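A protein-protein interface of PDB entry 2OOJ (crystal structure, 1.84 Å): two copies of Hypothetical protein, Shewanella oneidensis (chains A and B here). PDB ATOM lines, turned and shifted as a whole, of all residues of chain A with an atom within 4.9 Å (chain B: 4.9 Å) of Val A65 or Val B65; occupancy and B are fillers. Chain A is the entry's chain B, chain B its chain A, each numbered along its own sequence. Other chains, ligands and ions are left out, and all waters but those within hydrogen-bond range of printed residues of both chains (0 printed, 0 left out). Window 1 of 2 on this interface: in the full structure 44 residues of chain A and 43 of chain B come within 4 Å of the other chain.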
ATOM      1  N   GLU A  50      10.298  20.269  15.786  1.00  0.00           N
ATOM      2  CA  GLU A  50       8.977  20.536  16.257  1.00  0.00           C
ATOM      3  C   GLU A  50       8.600  21.969  15.969  1.00  0.00           C
ATOM      4  O   GLU A  50       9.459  22.813  15.769  1.00  0.00           O
ATOM      5  CB  GLU A  50       8.850  20.248  17.750  1.00  0.00           C
ATOM      6  CG  GLU A  50       9.122  18.808  18.084  1.00  0.00           C
ATOM      7  CD  GLU A  50       8.861  18.496  19.543  1.00  0.00           C
ATOM      8  OE1 GLU A  50       7.672  18.352  19.892  1.00  0.00           O
ATOM      9  OE2 GLU A  50       9.826  18.452  20.332  1.00  0.00           O
ATOM     10  N   MET A  51       7.292  22.194  15.934  1.00  0.00           N
ATOM     11  CA  MET A  51       6.685  23.486  15.778  1.00  0.00           C
ATOM     12  C   MET A  51       5.691  23.679  16.911  1.00  0.00           C
ATOM     13  O   MET A  51       5.118  22.714  17.428  1.00  0.00           O
ATOM     14  CB  MET A  51       5.947  23.509  14.450  1.00  0.00           C
ATOM     15  CG  MET A  51       5.067  24.724  14.222  1.00  0.00           C
ATOM     16  SD  MET A  51       3.971  24.515  12.558  1.00  0.00           S
ATOM     17  CE  MET A  51       4.032  22.794  12.489  1.00  0.00           C
ATOM     18  N   LEU A  52       5.504  24.933  17.290  1.00  0.00           N
ATOM     19  CA  LEU A  52       4.502  25.374  18.254  1.00  0.00           C
ATOM     20  C   LEU A  52       3.695  26.400  17.475  1.00  0.00           C
ATOM     21  O   LEU A  52       4.261  27.150  16.700  1.00  0.00           O
ATOM     22  CB  LEU A  52       5.166  26.014  19.468  1.00  0.00           C
ATOM     23  CG  LEU A  52       6.187  25.145  20.187  1.00  0.00           C
ATOM     24  CD1 LEU A  52       6.898  25.968  21.259  1.00  0.00           C
ATOM     25  CD2 LEU A  52       5.508  23.875  20.768  1.00  0.00           C
ATOM     26  N   GLY A  63       0.324  32.614  14.728  1.00  0.00           N
ATOM     27  CA  GLY A  63       1.803  32.636  14.826  1.00  0.00           C
ATOM     28  C   GLY A  63       2.298  31.231  14.918  1.00  0.00           C
ATOM     29  O   GLY A  63       1.542  30.351  15.332  1.00  0.00           O
ATOM     30  N   TYR A  64       3.533  30.987  14.459  1.00  0.00           N
ATOM     31  CA  TYR A  64       4.173  29.730  14.746  1.00  0.00           C
ATOM     32  C   TYR A  64       5.698  29.949  14.894  1.00  0.00           C
ATOM     33  O   TYR A  64       6.246  30.958  14.432  1.00  0.00           O
ATOM     34  CB  TYR A  64       3.854  28.724  13.655  1.00  0.00           C
ATOM     35  CG  TYR A  64       4.771  28.733  12.460  1.00  0.00           C
ATOM     36  CD1 TYR A  64       4.559  29.563  11.378  1.00  0.00           C
ATOM     37  CD2 TYR A  64       5.853  27.872  12.420  1.00  0.00           C
ATOM     38  CE1 TYR A  64       5.451  29.539  10.270  1.00  0.00           C
ATOM     39  CE2 TYR A  64       6.721  27.840  11.364  1.00  0.00           C
ATOM     40  CZ  TYR A  64       6.523  28.668  10.287  1.00  0.00           C
ATOM     41  OH  TYR A  64       7.440  28.580   9.230  1.00  0.00           O
ATOM     42  N   VAL A  65       6.317  29.010  15.567  1.00  0.00           N
ATOM     43  CA  VAL A  65       7.789  28.916  15.717  1.00  0.00           C
ATOM     44  C   VAL A  65       8.141  27.433  15.539  1.00  0.00           C
ATOM     45  O   VAL A  65       7.256  26.581  15.652  1.00  0.00           O
ATOM     46  CB  VAL A  65       8.271  29.449  17.062  1.00  0.00           C
ATOM     47  CG1 VAL A  65       7.874  30.875  17.259  1.00  0.00           C
ATOM     48  CG2 VAL A  65       7.810  28.611  18.270  1.00  0.00           C
ATOM     49  N   ALA A  66       9.395  27.147  15.208  1.00  0.00           N
ATOM     50  CA  ALA A  66       9.866  25.786  15.003  1.00  0.00           C
ATOM     51  C   ALA A  66      11.384  25.805  15.063  1.00  0.00           C
ATOM     52  O   ALA A  66      11.974  26.829  14.778  1.00  0.00           O
ATOM     53  CB  ALA A  66       9.398  25.280  13.648  1.00  0.00           C
ATOM     54  N   ILE A  67      11.972  24.659  15.409  1.00  0.00           N
ATOM     55  CA  ILE A  67      13.397  24.368  15.308  1.00  0.00           C
ATOM     56  C   ILE A  67      13.505  22.985  14.715  1.00  0.00           C
ATOM     57  O   ILE A  67      12.834  22.054  15.154  1.00  0.00           O
ATOM     58  CB  ILE A  67      14.090  24.403  16.699  1.00  0.00           C
ATOM     59  CG1 ILE A  67      14.144  25.872  17.170  1.00  0.00           C
ATOM     60  CG2 ILE A  67      15.495  23.825  16.678  1.00  0.00           C
ATOM     61  CD1 ILE A  67      14.866  26.080  18.477  1.00  0.00           C
ATOM     62  N   GLN A  84      15.668  27.708  12.299  1.00  0.00           N
ATOM     63  CA  GLN A  84      14.820  28.295  13.337  1.00  0.00           C
ATOM     64  C   GLN A  84      13.860  29.223  12.699  1.00  0.00           C
ATOM     65  O   GLN A  84      14.281  30.099  11.926  1.00  0.00           O
ATOM     66  CB  GLN A  84      15.676  29.029  14.373  1.00  0.00           C
ATOM     67  CG  GLN A  84      14.858  29.522  15.621  1.00  0.00           C
ATOM     68  CD  GLN A  84      15.765  29.963  16.747  1.00  0.00           C
ATOM     69  OE1 GLN A  84      16.545  29.167  17.271  1.00  0.00           O
ATOM     70  NE2 GLN A  84      15.637  31.218  17.161  1.00  0.00           N
ATOM     71  N   HIS A  85      12.565  28.975  12.946  1.00  0.00           N
ATOM     72  CA  HIS A  85      11.466  29.681  12.320  1.00  0.00           C
ATOM     73  C   HIS A  85      10.678  30.573  13.293  1.00  0.00           C
ATOM     74  O   HIS A  85      10.359  30.190  14.415  1.00  0.00           O
ATOM     75  CB  HIS A  85      10.395  28.709  11.771  1.00  0.00           C
ATOM     76  CG  HIS A  85      10.906  27.567  10.949  1.00  0.00           C
ATOM     77  ND1 HIS A  85      10.298  27.206   9.768  1.00  0.00           N
ATOM     78  CD2 HIS A  85      11.878  26.647  11.167  1.00  0.00           C
ATOM     79  CE1 HIS A  85      10.879  26.117   9.292  1.00  0.00           C
ATOM     80  NE2 HIS A  85      11.856  25.769  10.113  1.00  0.00           N
ATOM     81  N   PHE A  86      10.264  31.737  12.811  1.00  0.00           N
ATOM     82  CA  PHE A  86       9.349  32.568  13.539  1.00  0.00           C
ATOM     83  C   PHE A  86       8.457  33.173  12.490  1.00  0.00           C
ATOM     84  O   PHE A  86       8.940  33.904  11.635  1.00  0.00           O
ATOM     85  CB  PHE A  86      10.118  33.646  14.262  1.00  0.00           C
ATOM     86  CG  PHE A  86       9.280  34.664  14.996  1.00  0.00           C
ATOM     87  CD1 PHE A  86       8.740  35.749  14.337  1.00  0.00           C
ATOM     88  CD2 PHE A  86       9.160  34.591  16.374  1.00  0.00           C
ATOM     89  CE1 PHE A  86       8.030  36.731  15.036  1.00  0.00           C
ATOM     90  CE2 PHE A  86       8.467  35.566  17.100  1.00  0.00           C
ATOM     91  CZ  PHE A  86       7.888  36.632  16.420  1.00  0.00           C
ATOM     92  N   GLU B  50       5.363  26.527  25.865  1.00  0.00           N
ATOM     93  CA  GLU B  50       6.540  25.676  25.663  1.00  0.00           C
ATOM     94  C   GLU B  50       7.597  26.440  24.925  1.00  0.00           C
ATOM     95  O   GLU B  50       7.300  27.425  24.252  1.00  0.00           O
ATOM     96  CB  GLU B  50       6.220  24.385  24.915  1.00  0.00           C
ATOM     97  CG  GLU B  50       5.274  23.470  25.697  1.00  0.00           C
ATOM     98  CD  GLU B  50       5.065  22.117  25.058  1.00  0.00           C
ATOM     99  OE1 GLU B  50       5.911  21.234  25.228  1.00  0.00           O
ATOM    100  OE2 GLU B  50       4.020  21.910  24.411  1.00  0.00           O
ATOM    101  N   MET B  51       8.835  25.991  25.121  1.00  0.00           N
ATOM    102  CA  MET B  51      10.006  26.548  24.470  1.00  0.00           C
ATOM    103  C   MET B  51      10.737  25.447  23.759  1.00  0.00           C
ATOM    104  O   MET B  51      10.793  24.333  24.258  1.00  0.00           O
ATOM    105  CB  MET B  51      10.909  27.148  25.543  1.00  0.00           C
ATOM    106  CG  MET B  51      12.293  27.404  25.090  1.00  0.00           C
ATOM    107  SD  MET B  51      13.294  28.152  26.606  1.00  0.00           S
ATOM    108  CE  MET B  51      12.845  29.893  26.362  1.00  0.00           C
ATOM    109  N   LEU B  52      11.313  25.732  22.596  1.00  0.00           N
ATOM    110  CA  LEU B  52      12.254  24.802  21.947  1.00  0.00           C
ATOM    111  C   LEU B  52      13.613  25.510  21.874  1.00  0.00           C
ATOM    112  O   LEU B  52      13.681  26.724  21.666  1.00  0.00           O
ATOM    113  CB  LEU B  52      11.814  24.412  20.528  1.00  0.00           C
ATOM    114  CG  LEU B  52      10.374  23.946  20.347  1.00  0.00           C
ATOM    115  CD1 LEU B  52       9.992  23.948  18.854  1.00  0.00           C
ATOM    116  CD2 LEU B  52      10.224  22.575  20.976  1.00  0.00           C
ATOM    117  N   GLY B  63      19.917  28.960  19.998  1.00  0.00           N
ATOM    118  CA  GLY B  63      18.654  29.567  19.595  1.00  0.00           C
ATOM    119  C   GLY B  63      17.528  29.052  20.468  1.00  0.00           C
ATOM    120  O   GLY B  63      17.568  27.916  20.943  1.00  0.00           O
ATOM    121  N   TYR B  64      16.537  29.890  20.691  1.00  0.00           N
ATOM    122  CA  TYR B  64      15.326  29.481  21.444  1.00  0.00           C
ATOM    123  C   TYR B  64      14.118  30.016  20.738  1.00  0.00           C
ATOM    124  O   TYR B  64      14.165  31.117  20.156  1.00  0.00           O
ATOM    125  CB  TYR B  64      15.364  30.066  22.872  1.00  0.00           C
ATOM    126  CG  TYR B  64      16.665  29.779  23.584  1.00  0.00           C
ATOM    127  CD1 TYR B  64      17.773  30.619  23.455  1.00  0.00           C
ATOM    128  CD2 TYR B  64      16.812  28.618  24.347  1.00  0.00           C
ATOM    129  CE1 TYR B  64      18.986  30.321  24.121  1.00  0.00           C
ATOM    130  CE2 TYR B  64      18.014  28.312  24.996  1.00  0.00           C
ATOM    131  CZ  TYR B  64      19.084  29.156  24.885  1.00  0.00           C
ATOM    132  OH  TYR B  64      20.232  28.840  25.562  1.00  0.00           O
ATOM    133  N   VAL B  65      12.999  29.297  20.824  1.00  0.00           N
ATOM    134  CA  VAL B  65      11.717  29.873  20.407  1.00  0.00           C
ATOM    135  C   VAL B  65      10.704  29.432  21.443  1.00  0.00           C
ATOM    136  O   VAL B  65      10.885  28.395  22.092  1.00  0.00           O
ATOM    137  CB  VAL B  65      11.257  29.421  18.990  1.00  0.00           C
ATOM    138  CG1 VAL B  65      12.239  29.948  17.865  1.00  0.00           C
ATOM    139  CG2 VAL B  65      11.182  27.888  18.914  1.00  0.00           C
ATOM    140  N   ALA B  66       9.611  30.160  21.534  1.00  0.00           N
ATOM    141  CA  ALA B  66       8.551  29.784  22.450  1.00  0.00           C
ATOM    142  C   ALA B  66       7.208  30.382  22.060  1.00  0.00           C
ATOM    143  O   ALA B  66       7.119  31.386  21.323  1.00  0.00           O
ATOM    144  CB  ALA B  66       8.959  30.189  23.909  1.00  0.00           C
ATOM    145  N   ILE B  67       6.151  29.752  22.550  1.00  0.00           N
ATOM    146  CA  ILE B  67       4.811  30.323  22.511  1.00  0.00           C
ATOM    147  C   ILE B  67       4.201  30.106  23.886  1.00  0.00           C
ATOM    148  O   ILE B  67       4.277  28.999  24.446  1.00  0.00           O
ATOM    149  CB  ILE B  67       3.922  29.687  21.420  1.00  0.00           C
ATOM    150  CG1 ILE B  67       4.323  30.178  20.025  1.00  0.00           C
ATOM    151  CG2 ILE B  67       2.453  30.030  21.605  1.00  0.00           C
ATOM    152  CD1 ILE B  67       3.536  29.554  18.894  1.00  0.00           C
ATOM    153  N   GLN B  84       4.835  35.299  21.505  1.00  0.00           N
ATOM    154  CA  GLN B  84       5.676  34.484  20.675  1.00  0.00           C
ATOM    155  C   GLN B  84       7.117  35.029  20.737  1.00  0.00           C
ATOM    156  O   GLN B  84       7.340  36.209  20.538  1.00  0.00           O
ATOM    157  CB  GLN B  84       5.138  34.495  19.257  1.00  0.00           C
ATOM    158  CG  GLN B  84       5.874  33.580  18.346  1.00  0.00           C
ATOM    159  CD  GLN B  84       5.142  33.326  17.085  1.00  0.00           C
ATOM    160  OE1 GLN B  84       3.984  32.875  17.117  1.00  0.00           O
ATOM    161  NE2 GLN B  84       5.781  33.631  15.946  1.00  0.00           N
ATOM    162  N   HIS B  85       8.046  34.127  20.971  1.00  0.00           N
ATOM    163  CA  HIS B  85       9.481  34.391  21.244  1.00  0.00           C
ATOM    164  C   HIS B  85      10.373  33.816  20.144  1.00  0.00           C
ATOM    165  O   HIS B  85      10.185  32.650  19.684  1.00  0.00           O
ATOM    166  CB  HIS B  85       9.954  33.674  22.495  1.00  0.00           C
ATOM    167  CG  HIS B  85       9.184  33.960  23.742  1.00  0.00           C
ATOM    168  ND1 HIS B  85       9.815  34.187  24.946  1.00  0.00           N
ATOM    169  CD2 HIS B  85       7.855  33.942  24.013  1.00  0.00           C
ATOM    170  CE1 HIS B  85       8.909  34.329  25.899  1.00  0.00           C
ATOM    171  NE2 HIS B  85       7.711  34.203  25.355  1.00  0.00           N
ATOM    172  N   PHE B  86      11.396  34.586  19.790  1.00  0.00           N
ATOM    173  CA  PHE B  86      12.476  34.154  18.900  1.00  0.00           C
ATOM    174  C   PHE B  86      13.738  34.783  19.472  1.00  0.00           C
ATOM    175  O   PHE B  86      13.803  35.985  19.575  1.00  0.00           O
ATOM    176  CB  PHE B  86      12.227  34.655  17.463  1.00  0.00           C
ATOM    177  CG  PHE B  86      13.317  34.331  16.459  1.00  0.00           C
ATOM    178  CD1 PHE B  86      14.477  35.091  16.385  1.00  0.00           C
ATOM    179  CD2 PHE B  86      13.143  33.319  15.537  1.00  0.00           C
ATOM    180  CE1 PHE B  86      15.460  34.802  15.436  1.00  0.00           C
ATOM    181  CE2 PHE B  86      14.109  33.036  14.585  1.00  0.00           C
ATOM    182  CZ  PHE B  86      15.279  33.779  14.560  1.00  0.00           C
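Among the printed residues, merely in contact across the chains: Glu A50 with Leu B52 (3.3 Å), Leu A52 with Glu B50 (3.4 Å), Leu A52 with Ile B67 (3.3 Å), Gly A63 with Gln B84 (3.2 Å), Val A65 with Val B65 (3.5 Å), Val A65 with Gln B84 (3.5 Å), Val A65 with His B85 (3.8 Å), Ile A67 with Leu B52 (3.5 Å), Ile A67 with Val B65 (3.98 Å), Gln A84 with Gly B63 (3.2 Å), Gln A84 with Val B65 (3.5 Å), Gln A84 with Phe B86 (3.5 Å), His A85 with Val B65 (3.9 Å), Phe A86 with Gln B84 (3.5 Å), Phe A86 with His B85 (3.97 Å) and Phe A86 with Phe B86 (3.3 Å).
Val A65 touches just these residues of chain B: Val B65 (3.5 Å), Gln B84 (3.5 Å) and His B85 (3.8 Å).
Printed residues of chain B within 4 Å of Gly A63: Gln B84.
Printed residues of chain A within 4 Å of Ile B67: Leu A52.
The side-chain amide nitrogen (NE2) of Gln A84 is in hydrogen-bond range of the backbone carbonyl oxygen (O) of Tyr B64, at 3.3 Å.
NE2 of Gln B84 is in hydrogen-bond range of O of Tyr A64 (3.1 Å).
The backbone carbonyl oxygen (O) of Ile B67 sits at hydrogen-bond distance from the backbone NH (N) of Glu B50, at 3.1 Å.
The backbone NH (N) of His B85 lies within hydrogen-bond range of the backbone carbonyl oxygen (O) of Ala B66.
N of Ile A67 sits at hydrogen-bond distance from O of Glu A50, at 3.1 Å.
The backbone carbonyl oxygen of Val A65 lies within hydrogen-bond range of the backbone NH of Leu A52.
The side-chain hydroxyl (OH) of Tyr A64 sits at hydrogen-bond distance from a ring nitrogen (ND1) of His A85 (3.2 Å).
O of Ala A66 lies within hydrogen-bond range of N of His A85.
Val A65 touches Gln B84, and with the chains exchanged Gln A84 touches Val B65.
Val A65 touches His B85, and with the chains exchanged His A85 touches Val B65.
Ile A67 touches Val B65, but with the chains exchanged Val A65 does not touch Ile B67 (4.2 Å).
Phe A86 touches its own counterpart, Phe B86.
11 positions are printed for both chains.
Of the 18 pairs that touch across the chains among the printed residues, 16 have their exchanged pair printed and touching as well.
Hydrophobic or aromatic side chains of chain A within 4 Å of the printed part of chain B: Leu A52, Val A65, Ile A67 and Phe A86.
Along chain A the printed residues that touch a printed residue of chain B span positions 50 to 86.
Of the 11 printed residues of chain B, 9 touch a printed residue of chain A.
Hydrophobic or aromatic side chains of chain B within 4 Å of the printed part of chain A: Leu B52, Val B65, Ile B67 and Phe B86.
Among the printed residues, no Asp or Glu carboxylate lies within 4 Å of a Lys or Arg side-chain nitrogen of the other chain.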
